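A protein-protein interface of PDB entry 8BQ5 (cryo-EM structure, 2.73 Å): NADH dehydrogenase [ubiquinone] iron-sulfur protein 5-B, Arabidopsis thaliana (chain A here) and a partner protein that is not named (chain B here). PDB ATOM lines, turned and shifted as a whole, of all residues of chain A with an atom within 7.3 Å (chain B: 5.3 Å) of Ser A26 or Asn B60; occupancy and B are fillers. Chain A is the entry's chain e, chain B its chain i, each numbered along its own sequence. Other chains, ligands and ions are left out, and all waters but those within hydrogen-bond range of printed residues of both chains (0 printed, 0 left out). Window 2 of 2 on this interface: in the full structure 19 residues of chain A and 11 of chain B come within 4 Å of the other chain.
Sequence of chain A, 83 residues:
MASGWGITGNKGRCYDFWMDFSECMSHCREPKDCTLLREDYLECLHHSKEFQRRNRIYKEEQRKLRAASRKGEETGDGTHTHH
The backbone carbonyl oxygen of Met A25 lies close to the indole nitrogen of Trp B54. The backbone carbonyl oxygen of Cys A28 is in hydrogen-bond range of the indole nitrogen of Trp B54 (3.4 Å).
The backbone NH of Asp A20 is in hydrogen-bond range of the side-chain carboxylate of Glu A23, 3.0 Å away. O of Glu A23 lies within hydrogen-bond range of OG of Ser A26, 2.7 Å away. O of Glu A23 lies within hydrogen-bond range of NE2 of His A27 (3.3 Å). O of Cys A24 is in hydrogen-bond range of SG of Cys A28 (3.3 Å). The backbone NH (N) of Met A25 sits at hydrogen-bond distance from the side-chain sulfur (SG) of Cys A34 (3.3 Å). A ring nitrogen (ND1) of His A27 sits at hydrogen-bond distance from the side-chain sulfur (SG) of Cys A28, 3.5 Å away.
Among the printed residues, merely in contact across the chains: Ser A26 with Asn B60, Ser A26 with Thr B55, Glu A23 with Leu B63, Ser A22 with Leu B63, Ser A26 with Leu B63, Arg A29 with Trp B54, Met A25 with Thr B55 and His A27 with Thr B55.
Of the printed residues of chain B, Cys A28 touches Trp B54 (3.4 Å). Of chain A, only Ser A26 comes within 4 Å of Asn B60. Printed residues of chain A within 4 Å of Leu B63: Ser A22 (3.5 Å), Glu A23 (3.4 Å) and Ser A26 (3.6 Å). The nearest residue of chain A that does not touch Asn B60 is Ser A22 (5.0 Å). The nearest printed residue of chain A that does not touch Trp B54 is Ser A26 (4.8 Å).
Of the 11 printed residues of chain B, 4 touch a printed residue of chain A. Printed residues of chain B that touch a printed residue of chain A: Trp B54, Thr B55, Asn B60 and Leu B63. Among the printed residues, 10 pairs touch across the chains. Among the printed residues, no Asp or Glu carboxylate lies within 4 Å of a Lys or Arg side-chain nitrogen of the other chain.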
ATOM      1  N   ASP A  20     -28.468  12.504  28.202  1.00  0.00           N
ATOM      2  CA  ASP A  20     -28.923  13.423  29.249  1.00  0.00           C
ATOM      3  C   ASP A  20     -27.764  14.232  29.827  1.00  0.00           C
ATOM      4  O   ASP A  20     -27.884  15.446  30.038  1.00  0.00           O
ATOM      5  CB  ASP A  20     -29.654  12.649  30.345  1.00  0.00           C
ATOM      6  CG  ASP A  20     -30.884  11.945  29.825  1.00  0.00           C
ATOM      7  OD1 ASP A  20     -30.878  11.533  28.649  1.00  0.00           O
ATOM      8  OD2 ASP A  20     -31.863  11.809  30.583  1.00  0.00           O
ATOM      9  N   PHE A  21     -26.618  13.581  30.044  1.00  0.00           N
ATOM     10  CA  PHE A  21     -25.415  14.309  30.439  1.00  0.00           C
ATOM     11  C   PHE A  21     -25.060  15.388  29.419  1.00  0.00           C
ATOM     12  O   PHE A  21     -24.706  16.516  29.788  1.00  0.00           O
ATOM     13  CB  PHE A  21     -24.254  13.328  30.607  1.00  0.00           C
ATOM     14  CG  PHE A  21     -22.931  13.985  30.873  1.00  0.00           C
ATOM     15  CD1 PHE A  21     -22.801  14.942  31.863  1.00  0.00           C
ATOM     16  CD2 PHE A  21     -21.815  13.653  30.120  1.00  0.00           C
ATOM     17  CE1 PHE A  21     -21.585  15.544  32.106  1.00  0.00           C
ATOM     18  CE2 PHE A  21     -20.596  14.255  30.358  1.00  0.00           C
ATOM     19  CZ  PHE A  21     -20.482  15.202  31.351  1.00  0.00           C
ATOM     20  N   SER A  22     -25.162  15.059  28.127  1.00  0.00           N
ATOM     21  CA  SER A  22     -24.735  15.989  27.084  1.00  0.00           C
ATOM     22  C   SER A  22     -25.689  17.176  26.953  1.00  0.00           C
ATOM     23  O   SER A  22     -25.243  18.323  26.829  1.00  0.00           O
ATOM     24  CB  SER A  22     -24.592  15.245  25.754  1.00  0.00           C
ATOM     25  OG  SER A  22     -23.558  14.281  25.804  1.00  0.00           O
ATOM     26  N   GLU A  23     -27.001  16.922  26.981  1.00  0.00           N
ATOM     27  CA  GLU A  23     -27.960  18.027  27.023  1.00  0.00           C
ATOM     28  C   GLU A  23     -27.742  18.914  28.240  1.00  0.00           C
ATOM     29  O   GLU A  23     -27.822  20.144  28.135  1.00  0.00           O
ATOM     30  CB  GLU A  23     -29.422  17.560  26.997  1.00  0.00           C
ATOM     31  CG  GLU A  23     -29.950  16.844  25.755  1.00  0.00           C
ATOM     32  CD  GLU A  23     -30.121  15.381  25.882  1.00  0.00           C
ATOM     33  OE1 GLU A  23     -31.112  14.784  25.469  1.00  0.00           O
ATOM     34  OE2 GLU A  23     -29.267  14.781  26.413  1.00  0.00           O
ATOM     35  N   CYS A  24     -27.486  18.317  29.407  1.00  0.00           N
ATOM     36  CA  CYS A  24     -27.203  19.130  30.586  1.00  0.00           C
ATOM     37  C   CYS A  24     -26.010  20.041  30.340  1.00  0.00           C
ATOM     38  O   CYS A  24     -26.094  21.259  30.533  1.00  0.00           O
ATOM     39  CB  CYS A  24     -26.951  18.236  31.801  1.00  0.00           C
ATOM     40  SG  CYS A  24     -26.580  19.120  33.351  1.00  0.00           S
ATOM     41  N   MET A  25     -24.890  19.470  29.896  1.00  0.00           N
ATOM     42  CA  MET A  25     -23.697  20.285  29.696  1.00  0.00           C
ATOM     43  C   MET A  25     -23.867  21.283  28.559  1.00  0.00           C
ATOM     44  O   MET A  25     -23.130  22.271  28.503  1.00  0.00           O
ATOM     45  CB  MET A  25     -22.484  19.385  29.450  1.00  0.00           C
ATOM     46  CG  MET A  25     -22.074  18.618  30.695  1.00  0.00           C
ATOM     47  SD  MET A  25     -20.815  19.403  31.724  1.00  0.00           S
ATOM     48  CE  MET A  25     -19.540  19.760  30.524  1.00  0.00           C
ATOM     49  N   SER A  26     -24.836  21.064  27.669  1.00  0.00           N
ATOM     50  CA  SER A  26     -25.059  21.954  26.538  1.00  0.00           C
ATOM     51  C   SER A  26     -25.556  23.338  26.933  1.00  0.00           C
ATOM     52  O   SER A  26     -25.543  24.234  26.084  1.00  0.00           O
ATOM     53  CB  SER A  26     -26.059  21.323  25.573  1.00  0.00           C
ATOM     54  OG  SER A  26     -27.386  21.674  25.921  1.00  0.00           O
ATOM     55  N   HIS A  27     -26.028  23.534  28.165  1.00  0.00           N
ATOM     56  CA  HIS A  27     -26.448  24.867  28.585  1.00  0.00           C
ATOM     57  C   HIS A  27     -26.035  25.252  29.997  1.00  0.00           C
ATOM     58  O   HIS A  27     -26.303  26.390  30.396  1.00  0.00           O
ATOM     59  CB  HIS A  27     -27.971  25.015  28.462  1.00  0.00           C
ATOM     60  CG  HIS A  27     -28.739  23.884  29.070  1.00  0.00           C
ATOM     61  ND1 HIS A  27     -28.745  23.631  30.425  1.00  0.00           N
ATOM     62  CD2 HIS A  27     -29.522  22.935  28.507  1.00  0.00           C
ATOM     63  CE1 HIS A  27     -29.503  22.578  30.671  1.00  0.00           C
ATOM     64  NE2 HIS A  27     -29.986  22.136  29.523  1.00  0.00           N
ATOM     65  N   CYS A  28     -25.401  24.372  30.764  1.00  0.00           N
ATOM     66  CA  CYS A  28     -24.954  24.706  32.110  1.00  0.00           C
ATOM     67  C   CYS A  28     -23.509  25.184  32.047  1.00  0.00           C
ATOM     68  O   CYS A  28     -22.611  24.417  31.685  1.00  0.00           O
ATOM     69  CB  CYS A  28     -25.094  23.504  33.041  1.00  0.00           C
ATOM     70  SG  CYS A  28     -26.800  22.946  33.262  1.00  0.00           S
ATOM     71  N   ARG A  29     -23.290  26.453  32.397  1.00  0.00           N
ATOM     72  CA  ARG A  29     -21.967  27.055  32.310  1.00  0.00           C
ATOM     73  C   ARG A  29     -21.005  26.538  33.373  1.00  0.00           C
ATOM     74  O   ARG A  29     -19.790  26.618  33.171  1.00  0.00           O
ATOM     75  CB  ARG A  29     -22.087  28.577  32.407  1.00  0.00           C
ATOM     76  CG  ARG A  29     -22.588  29.233  31.126  1.00  0.00           C
ATOM     77  CD  ARG A  29     -22.646  30.747  31.250  1.00  0.00           C
ATOM     78  NE  ARG A  29     -23.545  31.180  32.314  1.00  0.00           N
ATOM     79  CZ  ARG A  29     -24.860  31.295  32.189  1.00  0.00           C
ATOM     80  NH1 ARG A  29     -25.474  31.011  31.052  1.00  0.00           N
ATOM     81  NH2 ARG A  29     -25.577  31.708  33.230  1.00  0.00           N
ATOM     82  N   CYS A  34     -23.852  19.488  36.273  1.00  0.00           N
ATOM     83  CA  CYS A  34     -24.163  18.240  35.591  1.00  0.00           C
ATOM     84  C   CYS A  34     -23.499  17.040  36.257  1.00  0.00           C
ATOM     85  O   CYS A  34     -23.346  15.990  35.627  1.00  0.00           O
ATOM     86  CB  CYS A  34     -23.750  18.331  34.123  1.00  0.00           C
ATOM     87  SG  CYS A  34     -24.614  19.622  33.211  1.00  0.00           S
ATOM     88  N   TRP B  54     -17.734  24.106  26.178  1.00  0.00           N
ATOM     89  CA  TRP B  54     -18.547  22.992  25.703  1.00  0.00           C
ATOM     90  C   TRP B  54     -19.978  23.410  25.388  1.00  0.00           C
ATOM     91  O   TRP B  54     -20.685  22.665  24.699  1.00  0.00           O
ATOM     92  CB  TRP B  54     -18.532  21.866  26.740  1.00  0.00           C
ATOM     93  CG  TRP B  54     -19.016  22.306  28.078  1.00  0.00           C
ATOM     94  CD1 TRP B  54     -20.299  22.300  28.520  1.00  0.00           C
ATOM     95  CD2 TRP B  54     -18.224  22.832  29.150  1.00  0.00           C
ATOM     96  NE1 TRP B  54     -20.364  22.788  29.802  1.00  0.00           N
ATOM     97  CE2 TRP B  54     -19.100  23.121  30.212  1.00  0.00           C
ATOM     98  CE3 TRP B  54     -16.860  23.085  29.314  1.00  0.00           C
ATOM     99  CZ2 TRP B  54     -18.657  23.648  31.421  1.00  0.00           C
ATOM    100  CZ3 TRP B  54     -16.422  23.609  30.512  1.00  0.00           C
ATOM    101  CH2 TRP B  54     -17.317  23.885  31.552  1.00  0.00           C
ATOM    102  N   THR B  55     -20.414  24.580  25.867  1.00  0.00           N
ATOM    103  CA  THR B  55     -21.742  25.095  25.546  1.00  0.00           C
ATOM    104  C   THR B  55     -21.814  25.640  24.121  1.00  0.00           C
ATOM    105  O   THR B  55     -22.906  25.728  23.547  1.00  0.00           O
ATOM    106  CB  THR B  55     -22.125  26.188  26.551  1.00  0.00           C
ATOM    107  OG1 THR B  55     -21.875  25.725  27.883  1.00  0.00           O
ATOM    108  CG2 THR B  55     -23.589  26.576  26.425  1.00  0.00           C
ATOM    109  N   PHE B  56     -20.659  26.038  23.566  1.00  0.00           N
ATOM    110  CA  PHE B  56     -20.623  26.650  22.209  1.00  0.00           C
ATOM    111  C   PHE B  56     -21.217  25.688  21.179  1.00  0.00           C
ATOM    112  O   PHE B  56     -21.021  24.466  21.309  1.00  0.00           O
ATOM    113  CB  PHE B  56     -19.216  27.091  21.804  1.00  0.00           C
ATOM    114  CG  PHE B  56     -18.519  28.053  22.737  1.00  0.00           C
ATOM    115  CD1 PHE B  56     -19.226  28.817  23.654  1.00  0.00           C
ATOM    116  CD2 PHE B  56     -17.143  28.198  22.690  1.00  0.00           C
ATOM    117  CE1 PHE B  56     -18.572  29.688  24.509  1.00  0.00           C
ATOM    118  CE2 PHE B  56     -16.490  29.076  23.539  1.00  0.00           C
ATOM    119  CZ  PHE B  56     -17.204  29.819  24.449  1.00  0.00           C
ATOM    120  N   GLU B  57     -21.861  26.233  20.146  1.00  0.00           N
ATOM    121  CA  GLU B  57     -22.599  25.415  19.187  1.00  0.00           C
ATOM    122  C   GLU B  57     -21.691  24.487  18.388  1.00  0.00           C
ATOM    123  O   GLU B  57     -22.110  23.388  18.011  1.00  0.00           O
ATOM    124  CB  GLU B  57     -23.401  26.310  18.239  1.00  0.00           C
ATOM    125  CG  GLU B  57     -24.684  26.869  18.845  1.00  0.00           C
ATOM    126  CD  GLU B  57     -24.428  27.848  19.974  1.00  0.00           C
ATOM    127  OE1 GLU B  57     -23.308  28.399  20.045  1.00  0.00           O
ATOM    128  OE2 GLU B  57     -25.342  28.060  20.798  1.00  0.00           O
ATOM    129  N   ARG B  58     -20.453  24.910  18.114  1.00  0.00           N
ATOM    130  CA  ARG B  58     -19.513  24.037  17.417  1.00  0.00           C
ATOM    131  C   ARG B  58     -19.253  22.756  18.200  1.00  0.00           C
ATOM    132  O   ARG B  58     -18.988  21.706  17.605  1.00  0.00           O
ATOM    133  CB  ARG B  58     -18.201  24.784  17.156  1.00  0.00           C
ATOM    134  CG  ARG B  58     -17.038  23.910  16.682  1.00  0.00           C
ATOM    135  CD  ARG B  58     -17.246  23.377  15.270  1.00  0.00           C
ATOM    136  NE  ARG B  58     -17.921  22.085  15.260  1.00  0.00           N
ATOM    137  CZ  ARG B  58     -18.360  21.472  14.168  1.00  0.00           C
ATOM    138  NH1 ARG B  58     -18.190  21.995  12.965  1.00  0.00           N
ATOM    139  NH2 ARG B  58     -18.986  20.304  14.287  1.00  0.00           N
ATOM    140  N   HIS B  59     -19.376  22.810  19.535  1.00  0.00           N
ATOM    141  CA  HIS B  59     -19.050  21.634  20.389  1.00  0.00           C
ATOM    142  C   HIS B  59     -20.314  20.841  20.730  1.00  0.00           C
ATOM    143  O   HIS B  59     -20.260  20.053  21.687  1.00  0.00           O
ATOM    144  CB  HIS B  59     -18.311  22.069  21.661  1.00  0.00           C
ATOM    145  CG  HIS B  59     -17.218  23.059  21.448  1.00  0.00           C
ATOM    146  ND1 HIS B  59     -17.447  24.339  20.985  1.00  0.00           N
ATOM    147  CD2 HIS B  59     -15.891  22.974  21.667  1.00  0.00           C
ATOM    148  CE1 HIS B  59     -16.308  24.988  20.900  1.00  0.00           C
ATOM    149  NE2 HIS B  59     -15.341  24.178  21.319  1.00  0.00           N
ATOM    150  N   ASN B  60     -21.392  21.030  19.972  1.00  0.00           N
ATOM    151  CA  ASN B  60     -22.663  20.358  20.230  1.00  0.00           C
ATOM    152  C   ASN B  60     -23.158  19.598  19.011  1.00  0.00           C
ATOM    153  O   ASN B  60     -24.365  19.473  18.785  1.00  0.00           O
ATOM    154  CB  ASN B  60     -23.702  21.373  20.685  1.00  0.00           C
ATOM    155  CG  ASN B  60     -23.769  21.493  22.182  1.00  0.00           C
ATOM    156  OD1 ASN B  60     -24.787  21.182  22.790  1.00  0.00           O
ATOM    157  ND2 ASN B  60     -22.675  21.933  22.794  1.00  0.00           N
ATOM    158  N   ALA B  61     -22.231  19.083  18.205  1.00  0.00           N
ATOM    159  CA  ALA B  61     -22.609  18.455  16.945  1.00  0.00           C
ATOM    160  C   ALA B  61     -23.423  17.184  17.163  1.00  0.00           C
ATOM    161  O   ALA B  61     -24.407  16.946  16.453  1.00  0.00           O
ATOM    162  CB  ALA B  61     -21.360  18.165  16.119  1.00  0.00           C
ATOM    163  N   GLN B  62     -23.032  16.350  18.133  1.00  0.00           N
ATOM    164  CA  GLN B  62     -23.759  15.101  18.351  1.00  0.00           C
ATOM    165  C   GLN B  62     -25.192  15.373  18.789  1.00  0.00           C
ATOM    166  O   GLN B  62     -26.117  14.656  18.391  1.00  0.00           O
ATOM    167  CB  GLN B  62     -23.040  14.223  19.381  1.00  0.00           C
ATOM    168  CG  GLN B  62     -23.872  13.026  19.854  1.00  0.00           C
ATOM    169  CD  GLN B  62     -23.077  12.008  20.656  1.00  0.00           C
ATOM    170  OE1 GLN B  62     -22.173  12.359  21.410  1.00  0.00           O
ATOM    171  NE2 GLN B  62     -23.420  10.735  20.496  1.00  0.00           N
ATOM    172  N   LEU B  63     -25.393  16.417  19.593  1.00  0.00           N
ATOM    173  CA  LEU B  63     -26.729  16.782  20.047  1.00  0.00           C
ATOM    174  C   LEU B  63     -27.653  17.175  18.905  1.00  0.00           C
ATOM    175  O   LEU B  63     -28.875  17.068  19.052  1.00  0.00           O
ATOM    176  CB  LEU B  63     -26.634  17.921  21.060  1.00  0.00           C
ATOM    177  CG  LEU B  63     -26.739  17.430  22.498  1.00  0.00           C
ATOM    178  CD1 LEU B  63     -26.109  18.404  23.467  1.00  0.00           C
ATOM    179  CD2 LEU B  63     -28.198  17.214  22.815  1.00  0.00           C
ATOM    180  N   ARG B  64     -27.111  17.633  17.776  1.00  0.00           N
ATOM    181  CA  ARG B  64     -27.941  17.955  16.623  1.00  0.00           C
ATOM    182  C   ARG B  64     -27.936  16.873  15.552  1.00  0.00           C
ATOM    183  O   ARG B  64     -28.906  16.774  14.795  1.00  0.00           O
ATOM    184  CB  ARG B  64     -27.499  19.284  15.991  1.00  0.00           C
ATOM    185  CG  ARG B  64     -26.986  20.313  16.984  1.00  0.00           C
ATOM    186  CD  ARG B  64     -27.249  21.742  16.513  1.00  0.00           C
ATOM    187  NE  ARG B  64     -26.283  22.209  15.524  1.00  0.00           N
ATOM    188  CZ  ARG B  64     -26.565  22.439  14.249  1.00  0.00           C
ATOM    189  NH1 ARG B  64     -27.777  22.233  13.760  1.00  0.00           N
ATOM    190  NH2 ARG B  64     -25.609  22.894  13.445  1.00  0.00           N
